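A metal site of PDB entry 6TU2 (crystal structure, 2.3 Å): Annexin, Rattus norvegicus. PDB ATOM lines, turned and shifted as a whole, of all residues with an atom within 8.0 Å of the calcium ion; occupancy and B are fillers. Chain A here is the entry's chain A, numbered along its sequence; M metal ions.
The calcium ion is bound by OE2 of Glu 78 (2.2 Å), O of Gly 36 (2.3 Å), O of Gly 38 (2.4 Å) and O of Met 34 (2.6 Å). The calcium ion has four donor atoms within binding distance.
Phe 37 touches the calcium ion (C to CA, 3.9 Å). Five residues have an atom within 4 Å of the calcium ion: Met 34, Gly 36, Phe 37, Gly 38 and Glu 78. The nearest printed residue that does not touch the calcium ion is Thr 39 (4.1 Å).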
ATOM      1  N   ARG A  31      -4.978  35.235  17.723  1.00  0.00           N
ATOM      2  CA  ARG A  31      -3.720  34.504  17.751  1.00  0.00           C
ATOM      3  C   ARG A  31      -3.226  34.325  19.186  1.00  0.00           C
ATOM      4  O   ARG A  31      -2.844  33.224  19.595  1.00  0.00           O
ATOM      5  CB  ARG A  31      -2.675  35.243  16.903  1.00  0.00           C
ATOM      6  CG  ARG A  31      -1.314  34.550  16.825  1.00  0.00           C
ATOM      7  CD  ARG A  31      -1.376  33.287  15.991  1.00  0.00           C
ATOM      8  NE  ARG A  31      -0.115  32.536  16.040  1.00  0.00           N
ATOM      9  CZ  ARG A  31      -0.020  31.223  16.219  1.00  0.00           C
ATOM     10  NH1 ARG A  31      -1.103  30.468  16.366  1.00  0.00           N
ATOM     11  NH2 ARG A  31       1.176  30.650  16.245  1.00  0.00           N
ATOM     12  N   LYS A  32      -3.243  35.405  19.966  1.00  0.00           N
ATOM     13  CA  LYS A  32      -2.787  35.328  21.347  1.00  0.00           C
ATOM     14  C   LYS A  32      -3.698  34.427  22.184  1.00  0.00           C
ATOM     15  O   LYS A  32      -3.238  33.796  23.133  1.00  0.00           O
ATOM     16  CB  LYS A  32      -2.716  36.720  21.956  1.00  0.00           C
ATOM     17  CG  LYS A  32      -1.475  37.510  21.540  1.00  0.00           C
ATOM     18  CD  LYS A  32      -1.613  38.998  21.838  1.00  0.00           C
ATOM     19  CE  LYS A  32      -0.366  39.758  21.401  1.00  0.00           C
ATOM     20  NZ  LYS A  32      -0.511  41.231  21.624  1.00  0.00           N
ATOM     21  N   ALA A  33      -4.983  34.357  21.830  1.00  0.00           N
ATOM     22  CA  ALA A  33      -5.903  33.505  22.586  1.00  0.00           C
ATOM     23  C   ALA A  33      -5.699  32.034  22.305  1.00  0.00           C
ATOM     24  O   ALA A  33      -6.125  31.193  23.108  1.00  0.00           O
ATOM     25  CB  ALA A  33      -7.352  33.899  22.280  1.00  0.00           C
ATOM     26  N   MET A  34      -5.058  31.685  21.184  1.00  0.00           N
ATOM     27  CA  MET A  34      -4.817  30.291  20.815  1.00  0.00           C
ATOM     28  C   MET A  34      -3.357  29.898  20.876  1.00  0.00           C
ATOM     29  O   MET A  34      -3.057  28.719  21.085  1.00  0.00           O
ATOM     30  CB  MET A  34      -5.337  30.020  19.402  1.00  0.00           C
ATOM     31  CG  MET A  34      -6.846  30.114  19.264  1.00  0.00           C
ATOM     32  SD  MET A  34      -7.413  29.703  17.612  1.00  0.00           S
ATOM     33  CE  MET A  34      -6.696  31.053  16.671  1.00  0.00           C
ATOM     34  N   LYS A  35      -2.439  30.845  20.684  1.00  0.00           N
ATOM     35  CA  LYS A  35      -1.019  30.532  20.732  1.00  0.00           C
ATOM     36  C   LYS A  35      -0.618  30.036  22.110  1.00  0.00           C
ATOM     37  O   LYS A  35      -1.056  30.580  23.140  1.00  0.00           O
ATOM     38  CB  LYS A  35      -0.205  31.779  20.363  1.00  0.00           C
ATOM     39  CG  LYS A  35       1.305  31.542  20.252  1.00  0.00           C
ATOM     40  CD  LYS A  35       2.042  32.800  19.783  1.00  0.00           C
ATOM     41  CE  LYS A  35       2.030  33.899  20.844  1.00  0.00           C
ATOM     42  NZ  LYS A  35       2.772  33.512  22.074  1.00  0.00           N
ATOM     43  N   GLY A  36       0.198  28.992  22.142  1.00  0.00           N
ATOM     44  CA  GLY A  36       0.670  28.436  23.388  1.00  0.00           C
ATOM     45  C   GLY A  36      -0.249  27.376  23.953  1.00  0.00           C
ATOM     46  O   GLY A  36      -1.243  26.976  23.334  1.00  0.00           O
ATOM     47  N   PHE A  37       0.087  26.916  25.153  1.00  0.00           N
ATOM     48  CA  PHE A  37      -0.729  25.920  25.819  1.00  0.00           C
ATOM     49  C   PHE A  37      -2.044  26.541  26.284  1.00  0.00           C
ATOM     50  O   PHE A  37      -2.148  27.749  26.497  1.00  0.00           O
ATOM     51  CB  PHE A  37       0.019  25.298  27.002  1.00  0.00           C
ATOM     52  CG  PHE A  37       0.075  26.169  28.227  1.00  0.00           C
ATOM     53  CD1 PHE A  37       1.197  26.935  28.493  1.00  0.00           C
ATOM     54  CD2 PHE A  37      -0.983  26.220  29.112  1.00  0.00           C
ATOM     55  CE1 PHE A  37       1.260  27.742  29.621  1.00  0.00           C
ATOM     56  CE2 PHE A  37      -0.937  27.020  30.236  1.00  0.00           C
ATOM     57  CZ  PHE A  37       0.190  27.777  30.492  1.00  0.00           C
ATOM     58  N   GLY A  38      -3.050  25.698  26.443  1.00  0.00           N
ATOM     59  CA  GLY A  38      -4.360  26.169  26.867  1.00  0.00           C
ATOM     60  C   GLY A  38      -5.010  27.078  25.843  1.00  0.00           C
ATOM     61  O   GLY A  38      -4.466  27.381  24.779  1.00  0.00           O
ATOM     62  N   THR A  39      -6.221  27.523  26.185  1.00  0.00           N
ATOM     63  CA  THR A  39      -7.021  28.354  25.295  1.00  0.00           C
ATOM     64  C   THR A  39      -7.749  29.415  26.109  1.00  0.00           C
ATOM     65  O   THR A  39      -8.188  29.144  27.231  1.00  0.00           O
ATOM     66  CB  THR A  39      -8.024  27.507  24.505  1.00  0.00           C
ATOM     67  OG1 THR A  39      -7.368  26.359  23.965  1.00  0.00           O
ATOM     68  CG2 THR A  39      -8.642  28.320  23.378  1.00  0.00           C
ATOM     69  N   ASP A  40      -7.884  30.598  25.528  1.00  0.00           N
ATOM     70  CA  ASP A  40      -8.596  31.715  26.155  1.00  0.00           C
ATOM     71  C   ASP A  40      -9.957  31.858  25.480  1.00  0.00           C
ATOM     72  O   ASP A  40     -10.171  32.705  24.617  1.00  0.00           O
ATOM     73  CB  ASP A  40      -7.769  32.994  26.060  1.00  0.00           C
ATOM     74  CG  ASP A  40      -8.398  34.167  26.793  1.00  0.00           C
ATOM     75  OD1 ASP A  40      -9.615  34.135  27.035  1.00  0.00           O
ATOM     76  OD2 ASP A  40      -7.663  35.116  27.114  1.00  0.00           O
ATOM     77  N   ASP A  74      -7.545  26.714  12.876  1.00  0.00           N
ATOM     78  CA  ASP A  74      -6.984  26.763  14.220  1.00  0.00           C
ATOM     79  C   ASP A  74      -8.077  26.696  15.284  1.00  0.00           C
ATOM     80  O   ASP A  74      -7.982  25.922  16.237  1.00  0.00           O
ATOM     81  CB  ASP A  74      -6.132  28.023  14.387  1.00  0.00           C
ATOM     82  CG  ASP A  74      -4.850  27.964  13.586  1.00  0.00           C
ATOM     83  OD1 ASP A  74      -4.679  26.998  12.811  1.00  0.00           O
ATOM     84  OD2 ASP A  74      -4.001  28.869  13.756  1.00  0.00           O
ATOM     85  N   SER A  77      -9.395  23.168  15.656  1.00  0.00           N
ATOM     86  CA  SER A  77      -8.565  22.271  16.446  1.00  0.00           C
ATOM     87  C   SER A  77      -8.398  22.737  17.893  1.00  0.00           C
ATOM     88  O   SER A  77      -8.052  21.920  18.759  1.00  0.00           O
ATOM     89  CB  SER A  77      -7.173  22.129  15.809  1.00  0.00           C
ATOM     90  OG  SER A  77      -6.451  23.338  15.920  1.00  0.00           O
ATOM     91  N   GLU A  78      -8.636  24.023  18.162  1.00  0.00           N
ATOM     92  CA  GLU A  78      -8.480  24.559  19.509  1.00  0.00           C
ATOM     93  C   GLU A  78      -9.736  24.360  20.347  1.00  0.00           C
ATOM     94  O   GLU A  78      -9.640  24.085  21.546  1.00  0.00           O
ATOM     95  CB  GLU A  78      -8.127  26.038  19.439  1.00  0.00           C
ATOM     96  CG  GLU A  78      -7.171  26.496  20.527  1.00  0.00           C
ATOM     97  CD  GLU A  78      -5.733  26.162  20.207  1.00  0.00           C
ATOM     98  OE1 GLU A  78      -5.485  25.459  19.212  1.00  0.00           O
ATOM     99  OE2 GLU A  78      -4.841  26.632  20.941  1.00  0.00           O
HETATM  100 CA    CA M   1      -3.474  26.735  22.668  1.00  0.00          CA
